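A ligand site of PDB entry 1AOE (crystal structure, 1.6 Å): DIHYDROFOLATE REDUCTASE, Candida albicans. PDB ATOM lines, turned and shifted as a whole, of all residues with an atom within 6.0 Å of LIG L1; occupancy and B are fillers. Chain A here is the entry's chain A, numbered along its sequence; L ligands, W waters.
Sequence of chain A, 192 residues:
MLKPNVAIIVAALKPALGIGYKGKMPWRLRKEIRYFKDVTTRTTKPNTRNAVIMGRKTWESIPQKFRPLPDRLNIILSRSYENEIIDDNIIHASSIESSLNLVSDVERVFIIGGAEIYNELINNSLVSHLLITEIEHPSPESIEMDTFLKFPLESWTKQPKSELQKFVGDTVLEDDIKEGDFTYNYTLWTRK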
ATOM      1  N   ILE A   9      20.710   7.540 -22.126  1.00  0.00           N
ATOM      2  CA  ILE A   9      21.469   6.487 -22.930  1.00  0.00           C
ATOM      3  C   ILE A   9      20.521   6.114 -24.046  1.00  0.00           C
ATOM      4  O   ILE A   9      19.347   5.768 -23.832  1.00  0.00           O
ATOM      5  CB  ILE A   9      21.909   5.298 -22.035  1.00  0.00           C
ATOM      6  CG1 ILE A   9      22.631   4.220 -22.895  1.00  0.00           C
ATOM      7  CG2 ILE A   9      20.723   4.669 -21.176  1.00  0.00           C
ATOM      8  CD1 ILE A   9      23.496   3.247 -21.992  1.00  0.00           C
ATOM      9  N   VAL A  10      21.064   6.129 -25.278  1.00  0.00           N
ATOM     10  CA  VAL A  10      20.288   5.836 -26.487  1.00  0.00           C
ATOM     11  C   VAL A  10      21.207   5.332 -27.630  1.00  0.00           C
ATOM     12  O   VAL A  10      22.411   5.613 -27.613  1.00  0.00           O
ATOM     13  CB  VAL A  10      19.547   7.153 -26.886  1.00  0.00           C
ATOM     14  CG1 VAL A  10      20.549   8.310 -27.156  1.00  0.00           C
ATOM     15  CG2 VAL A  10      18.579   7.033 -28.064  1.00  0.00           C
ATOM     16  N   ALA A  11      20.542   4.593 -28.524  1.00  0.00           N
ATOM     17  CA  ALA A  11      21.230   4.124 -29.756  1.00  0.00           C
ATOM     18  C   ALA A  11      20.533   4.795 -30.950  1.00  0.00           C
ATOM     19  O   ALA A  11      19.298   4.669 -31.080  1.00  0.00           O
ATOM     20  CB  ALA A  11      21.030   2.597 -29.856  1.00  0.00           C
ATOM     21  N   MET A  25      12.446  -1.128 -32.155  1.00  0.00           N
ATOM     22  CA  MET A  25      13.780  -0.636 -32.613  1.00  0.00           C
ATOM     23  C   MET A  25      13.946  -1.181 -34.040  1.00  0.00           C
ATOM     24  O   MET A  25      13.503  -2.300 -34.356  1.00  0.00           O
ATOM     25  CB  MET A  25      14.931  -0.959 -31.714  1.00  0.00           C
ATOM     26  CG  MET A  25      14.800  -0.246 -30.378  1.00  0.00           C
ATOM     27  SD  MET A  25      16.115  -0.802 -29.288  1.00  0.00           S
ATOM     28  CE  MET A  25      17.533   0.073 -29.945  1.00  0.00           C
ATOM     29  N   GLU A  32      25.257  -4.563 -28.693  1.00  0.00           N
ATOM     30  CA  GLU A  32      24.756  -3.241 -28.193  1.00  0.00           C
ATOM     31  C   GLU A  32      23.798  -3.437 -27.059  1.00  0.00           C
ATOM     32  O   GLU A  32      23.931  -2.733 -26.027  1.00  0.00           O
ATOM     33  CB  GLU A  32      24.066  -2.457 -29.340  1.00  0.00           C
ATOM     34  CG  GLU A  32      24.134  -0.920 -29.213  1.00  0.00           C
ATOM     35  CD  GLU A  32      23.277  -0.305 -28.151  1.00  0.00           C
ATOM     36  OE1 GLU A  32      22.175  -0.773 -27.899  1.00  0.00           O
ATOM     37  OE2 GLU A  32      23.750   0.707 -27.589  1.00  0.00           O
ATOM     38  N   ILE A  33      22.878  -4.403 -27.162  1.00  0.00           N
ATOM     39  CA  ILE A  33      21.940  -4.696 -26.023  1.00  0.00           C
ATOM     40  C   ILE A  33      22.739  -5.132 -24.770  1.00  0.00           C
ATOM     41  O   ILE A  33      22.368  -4.781 -23.655  1.00  0.00           O
ATOM     42  CB  ILE A  33      20.905  -5.799 -26.468  1.00  0.00           C
ATOM     43  CG1 ILE A  33      20.134  -5.400 -27.718  1.00  0.00           C
ATOM     44  CG2 ILE A  33      20.049  -6.347 -25.305  1.00  0.00           C
ATOM     45  CD1 ILE A  33      19.049  -4.344 -27.673  1.00  0.00           C
ATOM     46  N   TYR A  35      25.884  -4.215 -23.980  1.00  0.00           N
ATOM     47  CA  TYR A  35      26.516  -2.989 -23.427  1.00  0.00           C
ATOM     48  C   TYR A  35      25.448  -2.202 -22.576  1.00  0.00           C
ATOM     49  O   TYR A  35      25.778  -1.739 -21.486  1.00  0.00           O
ATOM     50  CB  TYR A  35      26.926  -2.119 -24.629  1.00  0.00           C
ATOM     51  CG  TYR A  35      27.274  -0.675 -24.339  1.00  0.00           C
ATOM     52  CD1 TYR A  35      28.532  -0.415 -23.801  1.00  0.00           C
ATOM     53  CD2 TYR A  35      26.381   0.394 -24.558  1.00  0.00           C
ATOM     54  CE1 TYR A  35      28.954   0.865 -23.512  1.00  0.00           C
ATOM     55  CE2 TYR A  35      26.802   1.703 -24.212  1.00  0.00           C
ATOM     56  CZ  TYR A  35      28.071   1.901 -23.715  1.00  0.00           C
ATOM     57  OH  TYR A  35      28.592   3.187 -23.432  1.00  0.00           O
ATOM     58  N   PHE A  36      24.305  -2.048 -23.200  1.00  0.00           N
ATOM     59  CA  PHE A  36      23.190  -1.308 -22.441  1.00  0.00           C
ATOM     60  C   PHE A  36      22.986  -1.963 -21.058  1.00  0.00           C
ATOM     61  O   PHE A  36      22.853  -1.275 -20.025  1.00  0.00           O
ATOM     62  CB  PHE A  36      21.953  -1.287 -23.319  1.00  0.00           C
ATOM     63  CG  PHE A  36      20.680  -0.878 -22.549  1.00  0.00           C
ATOM     64  CD1 PHE A  36      20.493   0.465 -22.229  1.00  0.00           C
ATOM     65  CD2 PHE A  36      19.830  -1.878 -22.085  1.00  0.00           C
ATOM     66  CE1 PHE A  36      19.347   0.831 -21.497  1.00  0.00           C
ATOM     67  CE2 PHE A  36      18.687  -1.509 -21.328  1.00  0.00           C
ATOM     68  CZ  PHE A  36      18.455  -0.154 -21.056  1.00  0.00           C
ATOM     69  N   THR A  58       7.377   2.712 -23.807  1.00  0.00           N
ATOM     70  CA  THR A  58       8.586   1.865 -23.762  1.00  0.00           C
ATOM     71  C   THR A  58       8.401   0.697 -22.778  1.00  0.00           C
ATOM     72  O   THR A  58       8.708  -0.453 -23.122  1.00  0.00           O
ATOM     73  CB  THR A  58       9.920   2.656 -23.511  1.00  0.00           C
ATOM     74  OG1 THR A  58      10.028   3.561 -24.701  1.00  0.00           O
ATOM     75  CG2 THR A  58      11.163   1.722 -23.530  1.00  0.00           C
ATOM     76  N   SER A  61       6.317  -1.976 -24.167  1.00  0.00           N
ATOM     77  CA  SER A  61       6.933  -2.655 -25.314  1.00  0.00           C
ATOM     78  C   SER A  61       7.776  -3.833 -24.863  1.00  0.00           C
ATOM     79  O   SER A  61       8.113  -4.687 -25.735  1.00  0.00           O
ATOM     80  CB  SER A  61       7.734  -1.660 -26.172  1.00  0.00           C
ATOM     81  OG  SER A  61       9.014  -1.385 -25.617  1.00  0.00           O
ATOM     82  N   ILE A  62       8.139  -3.940 -23.617  1.00  0.00           N
ATOM     83  CA  ILE A  62       8.967  -5.068 -23.089  1.00  0.00           C
ATOM     84  C   ILE A  62       7.917  -6.149 -22.711  1.00  0.00           C
ATOM     85  O   ILE A  62       6.924  -5.846 -22.045  1.00  0.00           O
ATOM     86  CB  ILE A  62       9.736  -4.606 -21.814  1.00  0.00           C
ATOM     87  CG1 ILE A  62      10.572  -3.338 -22.120  1.00  0.00           C
ATOM     88  CG2 ILE A  62      10.573  -5.752 -21.164  1.00  0.00           C
ATOM     89  CD1 ILE A  62      11.137  -2.587 -20.912  1.00  0.00           C
ATOM     90  N   LEU A  69      13.082  -4.615 -15.630  1.00  0.00           N
ATOM     91  CA  LEU A  69      14.478  -5.049 -16.004  1.00  0.00           C
ATOM     92  C   LEU A  69      15.196  -5.351 -14.690  1.00  0.00           C
ATOM     93  O   LEU A  69      15.216  -4.591 -13.718  1.00  0.00           O
ATOM     94  CB  LEU A  69      15.112  -3.884 -16.782  1.00  0.00           C
ATOM     95  CG  LEU A  69      14.391  -3.408 -18.007  1.00  0.00           C
ATOM     96  CD1 LEU A  69      15.157  -2.145 -18.484  1.00  0.00           C
ATOM     97  CD2 LEU A  69      14.323  -4.468 -19.073  1.00  0.00           C
ATOM     98  N   ILE A 111      18.078   7.721 -18.110  1.00  0.00           N
ATOM     99  CA  ILE A 111      16.854   7.823 -18.905  1.00  0.00           C
ATOM    100  C   ILE A 111      17.054   6.896 -20.152  1.00  0.00           C
ATOM    101  O   ILE A 111      18.007   7.110 -20.907  1.00  0.00           O
ATOM    102  CB  ILE A 111      16.566   9.291 -19.404  1.00  0.00           C
ATOM    103  CG1 ILE A 111      16.228  10.125 -18.114  1.00  0.00           C
ATOM    104  CG2 ILE A 111      15.390   9.301 -20.439  1.00  0.00           C
ATOM    105  CD1 ILE A 111      16.336  11.674 -18.449  1.00  0.00           C
ATOM    106  N   ILE A 112      16.150   5.921 -20.239  1.00  0.00           N
ATOM    107  CA  ILE A 112      16.263   4.902 -21.269  1.00  0.00           C
ATOM    108  C   ILE A 112      15.336   4.927 -22.440  1.00  0.00           C
ATOM    109  O   ILE A 112      15.342   3.989 -23.299  1.00  0.00           O
ATOM    110  CB  ILE A 112      16.442   3.478 -20.597  1.00  0.00           C
ATOM    111  CG1 ILE A 112      15.022   2.998 -20.084  1.00  0.00           C
ATOM    112  CG2 ILE A 112      17.564   3.489 -19.565  1.00  0.00           C
ATOM    113  CD1 ILE A 112      14.933   1.432 -19.868  1.00  0.00           C
ATOM    114  N   GLY A 113      14.486   5.956 -22.544  1.00  0.00           N
ATOM    115  CA  GLY A 113      13.580   6.102 -23.682  1.00  0.00           C
ATOM    116  C   GLY A 113      12.145   6.239 -23.233  1.00  0.00           C
ATOM    117  O   GLY A 113      11.841   6.167 -22.047  1.00  0.00           O
ATOM    118  N   TYR A 118      12.805  11.278 -24.381  1.00  0.00           N
ATOM    119  CA  TYR A 118      14.115  11.835 -24.747  1.00  0.00           C
ATOM    120  C   TYR A 118      14.063  13.334 -25.172  1.00  0.00           C
ATOM    121  O   TYR A 118      14.872  14.139 -24.712  1.00  0.00           O
ATOM    122  CB  TYR A 118      14.764  11.077 -25.894  1.00  0.00           C
ATOM    123  CG  TYR A 118      15.293   9.694 -25.603  1.00  0.00           C
ATOM    124  CD1 TYR A 118      16.136   9.420 -24.515  1.00  0.00           C
ATOM    125  CD2 TYR A 118      15.054   8.709 -26.579  1.00  0.00           C
ATOM    126  CE1 TYR A 118      16.664   8.150 -24.320  1.00  0.00           C
ATOM    127  CE2 TYR A 118      15.568   7.430 -26.423  1.00  0.00           C
ATOM    128  CZ  TYR A 118      16.393   7.190 -25.318  1.00  0.00           C
ATOM    129  OH  TYR A 118      16.930   5.922 -25.187  1.00  0.00           O
ATOM    130  N   LEU A 131      24.888   9.340 -23.333  1.00  0.00           N
ATOM    131  CA  LEU A 131      25.649   8.126 -23.834  1.00  0.00           C
ATOM    132  C   LEU A 131      24.951   7.735 -25.114  1.00  0.00           C
ATOM    133  O   LEU A 131      23.838   7.143 -25.108  1.00  0.00           O
ATOM    134  CB  LEU A 131      25.645   7.053 -22.740  1.00  0.00           C
ATOM    135  CG  LEU A 131      26.580   7.165 -21.558  1.00  0.00           C
ATOM    136  CD1 LEU A 131      26.402   5.940 -20.629  1.00  0.00           C
ATOM    137  CD2 LEU A 131      28.036   7.195 -21.964  1.00  0.00           C
ATOM    138  N   THR A 133      24.964   5.701 -28.633  1.00  0.00           N
ATOM    139  CA  THR A 133      25.603   4.680 -29.552  1.00  0.00           C
ATOM    140  C   THR A 133      25.325   5.225 -30.976  1.00  0.00           C
ATOM    141  O   THR A 133      24.168   5.273 -31.413  1.00  0.00           O
ATOM    142  CB  THR A 133      25.006   3.250 -29.363  1.00  0.00           C
ATOM    143  OG1 THR A 133      25.233   2.856 -27.979  1.00  0.00           O
ATOM    144  CG2 THR A 133      25.697   2.251 -30.348  1.00  0.00           C
HETATM  145  C1  LIG L   1      19.219   0.110 -25.815  1.00  0.00           C
HETATM  146  C2  LIG L   1      18.362   0.868 -25.024  1.00  0.00           C
HETATM  147  C3  LIG L   1      18.848   2.246 -24.690  1.00  0.00           C
HETATM  148  N1  LIG L   1      20.023   2.643 -25.032  1.00  0.00           N
HETATM  149  C4  LIG L   1      20.885   1.913 -25.729  1.00  0.00           C
HETATM  150  N2  LIG L   1      20.513   0.629 -26.154  1.00  0.00           N
HETATM  151  N3  LIG L   1      18.115   3.121 -24.005  1.00  0.00           N
HETATM  152  C5  LIG L   1      18.896  -1.232 -26.165  1.00  0.00           C
HETATM  153  C6  LIG L   1      17.660  -1.743 -25.784  1.00  0.00           C
HETATM  154  C7  LIG L   1      16.727  -1.001 -25.058  1.00  0.00           C
HETATM  155  C8  LIG L   1      17.126   0.314 -24.681  1.00  0.00           C
HETATM  156  C9  LIG L   1      15.973   0.749 -23.913  1.00  0.00           C
HETATM  157  C10 LIG L   1      15.119  -0.305 -23.971  1.00  0.00           C
HETATM  158  N4  LIG L   1      15.605  -1.284 -24.584  1.00  0.00           N
HETATM  159  N5  LIG L   1      22.105   2.311 -26.042  1.00  0.00           N
HETATM  160  C11 LIG L   1      14.814  -2.563 -24.749  1.00  0.00           C
HETATM  161  C12 LIG L   1      13.397  -2.376 -25.330  1.00  0.00           C
HETATM  162  C13 LIG L   1      13.324  -1.427 -26.531  1.00  0.00           C
HETATM  163  C14 LIG L   1      14.771  -3.307 -23.375  1.00  0.00           C
HETATM  164  C15 LIG L   1      16.117  -3.749 -22.844  1.00  0.00           C
HETATM  165  P1  LG2 L   2       7.756   6.731 -24.736  1.00  0.00           P
HETATM  166  O1  LG2 L   2       8.619   7.946 -24.651  1.00  0.00           O
HETATM  167  O2  LG2 L   2       8.440   5.503 -24.267  1.00  0.00           O
HETATM  168  O3  LG2 L   2       6.413   6.913 -23.851  1.00  0.00           O
HETATM  169  C1  LG2 L   2       5.586   8.108 -24.091  1.00  0.00           C
HETATM  170  C2  LG2 L   2       4.656   8.157 -22.840  1.00  0.00           C
HETATM  171  O4  LG2 L   2       5.453   8.533 -21.719  1.00  0.00           O
HETATM  172  C3  LG2 L   2       3.568   9.256 -22.971  1.00  0.00           C
HETATM  173  O5  LG2 L   2       2.485   8.740 -23.701  1.00  0.00           O
HETATM  174  C4  LG2 L   2       3.286   9.493 -21.441  1.00  0.00           C
HETATM  175  O6  LG2 L   2       2.510   8.530 -20.794  1.00  0.00           O
HETATM  176  C5  LG2 L   2       4.687   9.416 -20.901  1.00  0.00           C
HETATM  177  N1  LG2 L   2       5.370  10.658 -20.903  1.00  0.00           N
HETATM  178  C6  LG2 L   2       6.049  11.223 -21.949  1.00  0.00           C
HETATM  179  N2  LG2 L   2       6.628  12.361 -21.619  1.00  0.00           N
HETATM  180  C7  LG2 L   2       6.282  12.529 -20.309  1.00  0.00           C
HETATM  181  C8  LG2 L   2       6.625  13.543 -19.392  1.00  0.00           C
HETATM  182  N3  LG2 L   2       7.364  14.587 -19.791  1.00  0.00           N
HETATM  183  N4  LG2 L   2       6.119  13.432 -18.128  1.00  0.00           N
HETATM  184  C9  LG2 L   2       5.330  12.346 -17.834  1.00  0.00           C
HETATM  185  N5  LG2 L   2       4.990  11.344 -18.608  1.00  0.00           N
HETATM  186  C10 LG2 L   2       5.533  11.493 -19.835  1.00  0.00           C
HETATM  187  O7  LG2 L   2       7.210   6.513 -26.156  1.00  0.00           O
HETATM  188  P2  LG2 L   2       7.401   6.894 -27.686  1.00  0.00           P
HETATM  189  O8  LG2 L   2       6.333   6.303 -28.509  1.00  0.00           O
HETATM  190  O9  LG2 L   2       7.616   8.337 -27.923  1.00  0.00           O
HETATM  191  O10 LG2 L   2       8.828   6.154 -28.029  1.00  0.00           O
HETATM  192  C11 LG2 L   2       8.774   4.743 -28.351  1.00  0.00           C
HETATM  193  C12 LG2 L   2       9.823   4.539 -29.456  1.00  0.00           C
HETATM  194  O11 LG2 L   2      11.128   4.737 -28.866  1.00  0.00           O
HETATM  195  C13 LG2 L   2       9.804   3.095 -29.999  1.00  0.00           C
HETATM  196  O12 LG2 L   2      10.042   3.128 -31.401  1.00  0.00           O
HETATM  197  C14 LG2 L   2      10.986   2.495 -29.189  1.00  0.00           C
HETATM  198  O13 LG2 L   2      11.492   1.318 -29.828  1.00  0.00           O
HETATM  199  C15 LG2 L   2      11.965   3.657 -29.250  1.00  0.00           C
HETATM  200  N6  LG2 L   2      13.100   3.535 -28.303  1.00  0.00           N
HETATM  201  C16 LG2 L   2      14.386   3.585 -28.871  1.00  0.00           C
HETATM  202  C17 LG2 L   2      15.466   3.413 -28.023  1.00  0.00           C
HETATM  203  C18 LG2 L   2      16.881   3.503 -28.674  1.00  0.00           C
HETATM  204  O14 LG2 L   2      17.850   3.514 -27.948  1.00  0.00           O
HETATM  205  N7  LG2 L   2      16.919   3.581 -30.045  1.00  0.00           N
HETATM  206  C19 LG2 L   2      15.371   3.206 -26.610  1.00  0.00           C
HETATM  207  C20 LG2 L   2      14.010   3.170 -26.174  1.00  0.00           C
HETATM  208  C21 LG2 L   2      12.905   3.285 -26.954  1.00  0.00           C
HETATM  209  P3  LG2 L   2       0.824   8.753 -20.859  1.00  0.00           P
HETATM  210  O15 LG2 L   2       0.467   7.580 -20.000  1.00  0.00           O
HETATM  211  O16 LG2 L   2       0.677  10.082 -20.213  1.00  0.00           O
HETATM  212  O17 LG2 L   2       0.472   8.702 -22.259  1.00  0.00           O
HETATM  213  O   HOH W   1      10.408  -0.691 -27.906  1.00  0.00           O
HETATM  214  O   HOH W   2      24.854   4.365 -25.674  1.00  0.00           O
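A nitrogen (N5) of LIG L1 sits at hydrogen-bond distance from the side-chain carboxylate of Glu 32 (2.8 Å).
O of Ile 9 lies within hydrogen-bond range of N3 of LIG L1, at 2.9 Å.
O of Ile 112 sits at hydrogen-bond distance from N3 of LIG L1 (3.0 Å).
The side-chain hydroxyl of Tyr 118 lies within hydrogen-bond range of a nitrogen (N3) of LIG L1 (3.3 Å).
An oxygen (O14) of LG2 L2 lies within hydrogen-bond range of the backbone NH (N) of Ala 11 (3.0 Å).
The backbone carbonyl oxygen of Ala 11 sits at hydrogen-bond distance from a nitrogen (N7) of LG2 L2 (2.8 Å).
N of Thr 58 is in hydrogen-bond range of O2 of LG2 L2, at 3.0 Å.
An oxygen (O2) of LG2 L2 lies within hydrogen-bond range of the side-chain hydroxyl (OG1) of Thr 58 (2.5 Å).
OE2 of Glu 32 lies within hydrogen-bond range of OG1 of Thr 133 (2.6 Å).
OH of Tyr 118 sits at hydrogen-bond distance from O of Ile 9 (2.8 Å).
N of Ile 9 is in hydrogen-bond range of O of Ile 111 (3.0 Å).
The backbone carbonyl oxygen (O) of Ile 112 lies within hydrogen-bond range of the side-chain hydroxyl (OH) of Tyr 118 (3.1 Å).
The backbone carbonyl oxygen (O) of Val 10 is in hydrogen-bond range of the backbone NH (N) of Thr 133 (2.8 Å).
The backbone NH (N) of Val 10 is in hydrogen-bond range of the backbone carbonyl oxygen (O) of Leu 131, at 3.0 Å.
CA of Val 10 touches N1 of LIG L1, 3.5 Å away.
N of Ala 11 touches N5 of LIG L1 (3.7 Å).
Met 25 touches LIG L1 (SD to C6, 3.9 Å).
CD1 of Ile 33 touches C5 of LIG L1 (3.5 Å).
Phe 36 touches LIG L1 (CD1 to C3, 3.5 Å).
Thr 133 touches LIG L1.
Hydrophobic or aromatic side chains within 4 Å of LIG L1: Ile 9, Ala 11, Met 25, Ile 33, Phe 36 and Ile 112.
Water W1 lies within hydrogen-bond range of the side-chain hydroxyl of Ser 61 (2.8 Å) and an oxygen (O13) of LG2 L2 (3.0 Å).
Water W2 lies within hydrogen-bond range of the side-chain hydroxyl (OG1) of Thr 133, the backbone carbonyl oxygen (O) of Leu 131, the backbone carbonyl oxygen (O) of Val 10 and a nitrogen (N5) of LIG L1.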
